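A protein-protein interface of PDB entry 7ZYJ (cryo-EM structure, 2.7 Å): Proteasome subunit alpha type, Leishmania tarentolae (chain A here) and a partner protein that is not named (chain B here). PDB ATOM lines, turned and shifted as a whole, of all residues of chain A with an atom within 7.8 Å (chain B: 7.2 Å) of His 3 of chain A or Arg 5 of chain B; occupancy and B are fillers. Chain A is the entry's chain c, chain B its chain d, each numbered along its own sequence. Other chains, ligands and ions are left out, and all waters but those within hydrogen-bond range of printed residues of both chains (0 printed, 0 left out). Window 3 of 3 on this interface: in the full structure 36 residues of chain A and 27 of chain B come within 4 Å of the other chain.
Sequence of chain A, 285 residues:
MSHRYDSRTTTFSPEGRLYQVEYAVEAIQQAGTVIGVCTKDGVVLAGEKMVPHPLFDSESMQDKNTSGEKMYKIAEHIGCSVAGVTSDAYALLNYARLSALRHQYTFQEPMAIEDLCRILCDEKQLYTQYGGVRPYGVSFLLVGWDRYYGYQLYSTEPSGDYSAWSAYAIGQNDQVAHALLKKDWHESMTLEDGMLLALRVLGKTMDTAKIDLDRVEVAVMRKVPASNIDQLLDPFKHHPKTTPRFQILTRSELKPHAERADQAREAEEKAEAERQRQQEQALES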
ATOM      1  N   SER A   2       5.810 -17.360   2.682  1.00  0.00           N
ATOM      2  CA  SER A   2       4.530 -16.682   2.515  1.00  0.00           C
ATOM      3  C   SER A   2       3.783 -16.583   3.840  1.00  0.00           C
ATOM      4  O   SER A   2       4.085 -17.305   4.790  1.00  0.00           O
ATOM      5  CB  SER A   2       3.670 -17.404   1.479  1.00  0.00           C
ATOM      6  OG  SER A   2       3.258 -18.672   1.953  1.00  0.00           O
ATOM      7  N   HIS A   3       2.799 -15.683   3.895  1.00  0.00           N
ATOM      8  CA  HIS A   3       2.050 -15.459   5.125  1.00  0.00           C
ATOM      9  C   HIS A   3       1.155 -16.636   5.490  1.00  0.00           C
ATOM     10  O   HIS A   3       0.677 -16.701   6.627  1.00  0.00           O
ATOM     11  CB  HIS A   3       1.211 -14.186   5.002  1.00  0.00           C
ATOM     12  CG  HIS A   3       0.003 -14.339   4.133  1.00  0.00           C
ATOM     13  ND1 HIS A   3      -1.213 -14.776   4.617  1.00  0.00           N
ATOM     14  CD2 HIS A   3      -0.179 -14.114   2.810  1.00  0.00           C
ATOM     15  CE1 HIS A   3      -2.089 -14.813   3.630  1.00  0.00           C
ATOM     16  NE2 HIS A   3      -1.489 -14.416   2.523  1.00  0.00           N
ATOM     17  N   ARG A   4       0.916 -17.561   4.558  1.00  0.00           N
ATOM     18  CA  ARG A   4       0.099 -18.731   4.859  1.00  0.00           C
ATOM     19  C   ARG A   4       0.713 -19.604   5.944  1.00  0.00           C
ATOM     20  O   ARG A   4      -0.021 -20.136   6.783  1.00  0.00           O
ATOM     21  CB  ARG A   4      -0.114 -19.571   3.600  1.00  0.00           C
ATOM     22  CG  ARG A   4      -0.826 -18.855   2.468  1.00  0.00           C
ATOM     23  CD  ARG A   4      -1.193 -19.837   1.369  1.00  0.00           C
ATOM     24  NE  ARG A   4      -2.282 -20.717   1.774  1.00  0.00           N
ATOM     25  CZ  ARG A   4      -2.669 -21.793   1.101  1.00  0.00           C
ATOM     26  NH1 ARG A   4      -2.065 -22.163  -0.015  1.00  0.00           N
ATOM     27  NH2 ARG A   4      -3.683 -22.516   1.564  1.00  0.00           N
ATOM     28  N   TYR A   5       2.034 -19.762   5.944  1.00  0.00           N
ATOM     29  CA  TYR A   5       2.721 -20.659   6.859  1.00  0.00           C
ATOM     30  C   TYR A   5       3.205 -19.957   8.121  1.00  0.00           C
ATOM     31  O   TYR A   5       3.898 -20.575   8.934  1.00  0.00           O
ATOM     32  CB  TYR A   5       3.891 -21.330   6.139  1.00  0.00           C
ATOM     33  CG  TYR A   5       3.526 -21.816   4.754  1.00  0.00           C
ATOM     34  CD1 TYR A   5       2.537 -22.774   4.573  1.00  0.00           C
ATOM     35  CD2 TYR A   5       4.155 -21.306   3.630  1.00  0.00           C
ATOM     36  CE1 TYR A   5       2.194 -23.218   3.313  1.00  0.00           C
ATOM     37  CE2 TYR A   5       3.820 -21.744   2.363  1.00  0.00           C
ATOM     38  CZ  TYR A   5       2.839 -22.700   2.211  1.00  0.00           C
ATOM     39  OH  TYR A   5       2.499 -23.138   0.952  1.00  0.00           O
ATOM     40  N   ASP A   6       2.863 -18.684   8.298  1.00  0.00           N
ATOM     41  CA  ASP A   6       3.218 -17.965   9.515  1.00  0.00           C
ATOM     42  C   ASP A   6       2.439 -18.541  10.693  1.00  0.00           C
ATOM     43  O   ASP A   6       1.212 -18.658  10.635  1.00  0.00           O
ATOM     44  CB  ASP A   6       2.928 -16.476   9.349  1.00  0.00           C
ATOM     45  CG  ASP A   6       3.450 -15.643  10.503  1.00  0.00           C
ATOM     46  OD1 ASP A   6       4.070 -16.210  11.426  1.00  0.00           O
ATOM     47  OD2 ASP A   6       3.242 -14.412  10.488  1.00  0.00           O
ATOM     48  N   SER A   7       3.155 -18.899  11.759  1.00  0.00           N
ATOM     49  CA  SER A   7       2.522 -19.504  12.923  1.00  0.00           C
ATOM     50  C   SER A   7       1.908 -18.478  13.867  1.00  0.00           C
ATOM     51  O   SER A   7       1.109 -18.857  14.730  1.00  0.00           O
ATOM     52  CB  SER A   7       3.535 -20.358  13.685  1.00  0.00           C
ATOM     53  OG  SER A   7       4.583 -19.557  14.198  1.00  0.00           O
ATOM     54  N   ARG A   8       2.263 -17.199  13.723  1.00  0.00           N
ATOM     55  CA  ARG A   8       1.716 -16.111  14.535  1.00  0.00           C
ATOM     56  C   ARG A   8       1.962 -16.367  16.026  1.00  0.00           C
ATOM     57  O   ARG A   8       1.041 -16.533  16.828  1.00  0.00           O
ATOM     58  CB  ARG A   8       0.225 -15.913  14.240  1.00  0.00           C
ATOM     59  CG  ARG A   8      -0.051 -15.032  13.038  1.00  0.00           C
ATOM     60  CD  ARG A   8      -1.537 -14.781  12.880  1.00  0.00           C
ATOM     61  NE  ARG A   8      -2.216 -15.908  12.255  1.00  0.00           N
ATOM     62  CZ  ARG A   8      -3.031 -16.737  12.891  1.00  0.00           C
ATOM     63  NH1 ARG A   8      -3.290 -16.598  14.181  1.00  0.00           N
ATOM     64  NH2 ARG A   8      -3.600 -17.732  12.218  1.00  0.00           N
ATOM     65  N   THR A  10       3.441 -14.326  18.339  1.00  0.00           N
ATOM     66  CA  THR A  10       3.126 -13.198  19.217  1.00  0.00           C
ATOM     67  C   THR A  10       1.732 -12.646  18.910  1.00  0.00           C
ATOM     68  O   THR A  10       1.554 -11.498  18.506  1.00  0.00           O
ATOM     69  CB  THR A  10       4.189 -12.113  19.090  1.00  0.00           C
ATOM     70  OG1 THR A  10       4.012 -11.406  17.857  1.00  0.00           O
ATOM     71  CG2 THR A  10       5.580 -12.725  19.122  1.00  0.00           C
ATOM     72  N   THR A  11       0.731 -13.498  19.115  1.00  0.00           N
ATOM     73  CA  THR A  11      -0.663 -13.125  18.932  1.00  0.00           C
ATOM     74  C   THR A  11      -1.482 -13.613  20.118  1.00  0.00           C
ATOM     75  O   THR A  11      -1.150 -14.611  20.762  1.00  0.00           O
ATOM     76  CB  THR A  11      -1.245 -13.702  17.633  1.00  0.00           C
ATOM     77  OG1 THR A  11      -0.885 -15.084  17.518  1.00  0.00           O
ATOM     78  CG2 THR A  11      -0.721 -12.944  16.427  1.00  0.00           C
ATOM     79  N   GLY A 132       7.935 -11.894  15.959  1.00  0.00           N
ATOM     80  CA  GLY A 132       7.291 -12.989  15.263  1.00  0.00           C
ATOM     81  C   GLY A 132       8.014 -14.311  15.357  1.00  0.00           C
ATOM     82  O   GLY A 132       7.770 -15.199  14.537  1.00  0.00           O
ATOM     83  N   SER B   2      12.270  -6.347   8.444  1.00  0.00           N
ATOM     84  CA  SER B   2      11.916  -7.012   9.692  1.00  0.00           C
ATOM     85  C   SER B   2      10.454  -7.443   9.691  1.00  0.00           C
ATOM     86  O   SER B   2       9.675  -7.029   8.833  1.00  0.00           O
ATOM     87  CB  SER B   2      12.193  -6.095  10.886  1.00  0.00           C
ATOM     88  OG  SER B   2      11.143  -5.161  11.066  1.00  0.00           O
ATOM     89  N   TYR B   3      10.093  -8.281  10.659  1.00  0.00           N
ATOM     90  CA  TYR B   3       8.727  -8.779  10.764  1.00  0.00           C
ATOM     91  C   TYR B   3       7.773  -7.642  11.104  1.00  0.00           C
ATOM     92  O   TYR B   3       7.836  -7.071  12.197  1.00  0.00           O
ATOM     93  CB  TYR B   3       8.658  -9.874  11.826  1.00  0.00           C
ATOM     94  CG  TYR B   3       7.309 -10.542  11.948  1.00  0.00           C
ATOM     95  CD1 TYR B   3       6.938 -11.563  11.086  1.00  0.00           C
ATOM     96  CD2 TYR B   3       6.410 -10.159  12.934  1.00  0.00           C
ATOM     97  CE1 TYR B   3       5.708 -12.179  11.197  1.00  0.00           C
ATOM     98  CE2 TYR B   3       5.178 -10.769  13.053  1.00  0.00           C
ATOM     99  CZ  TYR B   3       4.833 -11.779  12.182  1.00  0.00           C
ATOM    100  OH  TYR B   3       3.606 -12.389  12.296  1.00  0.00           O
ATOM    101  N   ASP B   4       6.888  -7.312  10.165  1.00  0.00           N
ATOM    102  CA  ASP B   4       5.904  -6.255  10.363  1.00  0.00           C
ATOM    103  C   ASP B   4       4.542  -6.687   9.836  1.00  0.00           C
ATOM    104  O   ASP B   4       3.783  -5.882   9.286  1.00  0.00           O
ATOM    105  CB  ASP B   4       6.358  -4.949   9.709  1.00  0.00           C
ATOM    106  CG  ASP B   4       6.316  -5.006   8.195  1.00  0.00           C
ATOM    107  OD1 ASP B   4       6.812  -5.996   7.618  1.00  0.00           O
ATOM    108  OD2 ASP B   4       5.776  -4.061   7.584  1.00  0.00           O
ATOM    109  N   ARG B   5       4.206  -7.960  10.012  1.00  0.00           N
ATOM    110  CA  ARG B   5       2.910  -8.457   9.571  1.00  0.00           C
ATOM    111  C   ARG B   5       1.791  -7.821  10.385  1.00  0.00           C
ATOM    112  O   ARG B   5       1.932  -7.586  11.588  1.00  0.00           O
ATOM    113  CB  ARG B   5       2.849  -9.979   9.695  1.00  0.00           C
ATOM    114  CG  ARG B   5       1.607 -10.597   9.072  1.00  0.00           C
ATOM    115  CD  ARG B   5       1.818 -12.061   8.737  1.00  0.00           C
ATOM    116  NE  ARG B   5       0.648 -12.642   8.089  1.00  0.00           N
ATOM    117  CZ  ARG B   5      -0.330 -13.270   8.729  1.00  0.00           C
ATOM    118  NH1 ARG B   5      -0.317 -13.411  10.044  1.00  0.00           N
ATOM    119  NH2 ARG B   5      -1.347 -13.768   8.031  1.00  0.00           N
ATOM    120  N   ALA B   6       0.675  -7.537   9.718  1.00  0.00           N
ATOM    121  CA  ALA B   6      -0.483  -6.969  10.394  1.00  0.00           C
ATOM    122  C   ALA B   6      -1.071  -7.992  11.356  1.00  0.00           C
ATOM    123  O   ALA B   6      -1.568  -9.040  10.932  1.00  0.00           O
ATOM    124  CB  ALA B   6      -1.527  -6.526   9.372  1.00  0.00           C
ATOM    125  N   ILE B   7      -1.015  -7.689  12.648  1.00  0.00           N
ATOM    126  CA  ILE B   7      -1.511  -8.582  13.688  1.00  0.00           C
ATOM    127  C   ILE B   7      -2.899  -8.172  14.155  1.00  0.00           C
ATOM    128  O   ILE B   7      -3.794  -9.008  14.279  1.00  0.00           O
ATOM    129  CB  ILE B   7      -0.511  -8.636  14.864  1.00  0.00           C
ATOM    130  CG1 ILE B   7       0.755  -9.384  14.448  1.00  0.00           C
ATOM    131  CG2 ILE B   7      -1.148  -9.285  16.083  1.00  0.00           C
ATOM    132  CD1 ILE B   7       1.746  -9.585  15.571  1.00  0.00           C
ATOM    133  N   THR B   8      -3.102  -6.883  14.412  1.00  0.00           N
ATOM    134  CA  THR B   8      -4.410  -6.359  14.783  1.00  0.00           C
ATOM    135  C   THR B   8      -5.135  -5.947  13.508  1.00  0.00           C
ATOM    136  O   THR B   8      -4.760  -4.965  12.860  1.00  0.00           O
ATOM    137  CB  THR B   8      -4.272  -5.181  15.743  1.00  0.00           C
ATOM    138  OG1 THR B   8      -3.468  -5.567  16.865  1.00  0.00           O
ATOM    139  CG2 THR B   8      -5.639  -4.735  16.237  1.00  0.00           C
ATOM    140  N   VAL B   9      -6.170  -6.702  13.143  1.00  0.00           N
ATOM    141  CA  VAL B   9      -6.926  -6.463  11.923  1.00  0.00           C
ATOM    142  C   VAL B   9      -8.411  -6.465  12.256  1.00  0.00           C
ATOM    143  O   VAL B   9      -8.845  -7.007  13.274  1.00  0.00           O
ATOM    144  CB  VAL B   9      -6.621  -7.510  10.827  1.00  0.00           C
ATOM    145  CG1 VAL B   9      -5.146  -7.490  10.463  1.00  0.00           C
ATOM    146  CG2 VAL B   9      -7.044  -8.896  11.285  1.00  0.00           C
ATOM    147  N   SER B 121       0.392  -1.182  15.072  1.00  0.00           N
ATOM    148  CA  SER B 121       1.748  -1.374  14.582  1.00  0.00           C
ATOM    149  C   SER B 121       1.913  -2.801  14.079  1.00  0.00           C
ATOM    150  O   SER B 121       1.564  -3.759  14.776  1.00  0.00           O
ATOM    151  CB  SER B 121       2.777  -1.081  15.675  1.00  0.00           C
ATOM    152  OG  SER B 121       2.772  -2.095  16.664  1.00  0.00           O
ATOM    153  N   GLY B 122       2.442  -2.937  12.867  1.00  0.00           N
ATOM    154  CA  GLY B 122       2.624  -4.252  12.279  1.00  0.00           C
ATOM    155  C   GLY B 122       3.714  -5.039  12.988  1.00  0.00           C
ATOM    156  O   GLY B 122       4.746  -4.500  13.385  1.00  0.00           O
ATOM    157  N   GLY B 123       3.469  -6.337  13.143  1.00  0.00           N
ATOM    158  CA  GLY B 123       4.431  -7.206  13.787  1.00  0.00           C
ATOM    159  C   GLY B 123       4.412  -7.179  15.296  1.00  0.00           C
ATOM    160  O   GLY B 123       5.339  -7.697  15.923  1.00  0.00           O
ATOM    161  N   SER B 124       3.384  -6.591  15.903  1.00  0.00           N
ATOM    162  CA  SER B 124       3.302  -6.494  17.352  1.00  0.00           C
ATOM    163  C   SER B 124       1.859  -6.645  17.802  1.00  0.00           C
ATOM    164  O   SER B 124       0.943  -6.119  17.164  1.00  0.00           O
ATOM    165  CB  SER B 124       3.866  -5.161  17.855  1.00  0.00           C
ATOM    166  OG  SER B 124       2.870  -4.153  17.856  1.00  0.00           O
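OD2 of Asp 6 of chain A sits at hydrogen-bond distance from OH of Tyr 3 of chain B.
OD2 of Asp 6 of chain A lies within salt-bridge range of NH1 of Arg 5 of chain B, 3.7 Å away.
The side-chain carboxylate (OD1) of Asp 6 of chain A sits at hydrogen-bond distance from the backbone NH (N) of Arg 8 of chain A (3.1 Å).
OG1 of Thr 11 of chain A sits at hydrogen-bond distance from O of Arg 8 of chain A, at 2.5 Å.
The backbone carbonyl oxygen of Arg 5 of chain B lies within hydrogen-bond range of the backbone NH of Gly 123 of chain B (2.5 Å).
His 3 of chain A touches Arg 5 of chain B.
CD of Arg 8 of chain A touches NH1 of Arg 5 of chain B, at 3.4 Å.
Thr 10 of chain A touches Ile 7 of chain B.
Thr 11 of chain A touches Ile 7 of chain B (CG2 to CG2, 3.7 Å).
Gly 132 of chain A touches Tyr 3 of chain B (CA to CD2, 3.8 Å).
Of chain B, only Arg 5 comes within 4 Å of His 3 of chain A.
Arg 5 of chain B touches just these residues of chain A: His 3 (3.5 Å), Asp 6 (3.3 Å) and Arg 8 (3.4 Å).
Of the printed residues of chain B, Thr 10 of chain A touches Ile 7.
Printed residues of chain B within 4 Å of Thr 11 of chain A: Ile 7 (3.7 Å).
Ser 121 of chain B touches none of the printed residues of chain A.
Ser 2 of chain A touches none of the printed residues of chain B.
The nearest residue of chain A that does not touch Arg 5 of chain B is Arg 4 of chain A (5.6 Å).
The nearest printed residue of chain A that does not touch Tyr 3 of chain B is Arg 8 of chain A (4.6 Å).
Of the 10 printed residues of chain A, 6 touch a printed residue of chain B.
Hydrophobic or aromatic side chains of chain A within 4 Å of the printed part of chain B: His 3.
Along chain A the printed residues that touch a printed residue of chain B span positions 3 to 132.
Of the 12 printed residues of chain B, 3 touch a printed residue of chain A.
Among the printed residues, 7 pairs touch across the chains.
Among the printed residues, Asp or Glu carboxylates within 4 Å of a Lys or Arg side-chain nitrogen of the other chain: Asp 6 of chain A with Arg 5 of chain B.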
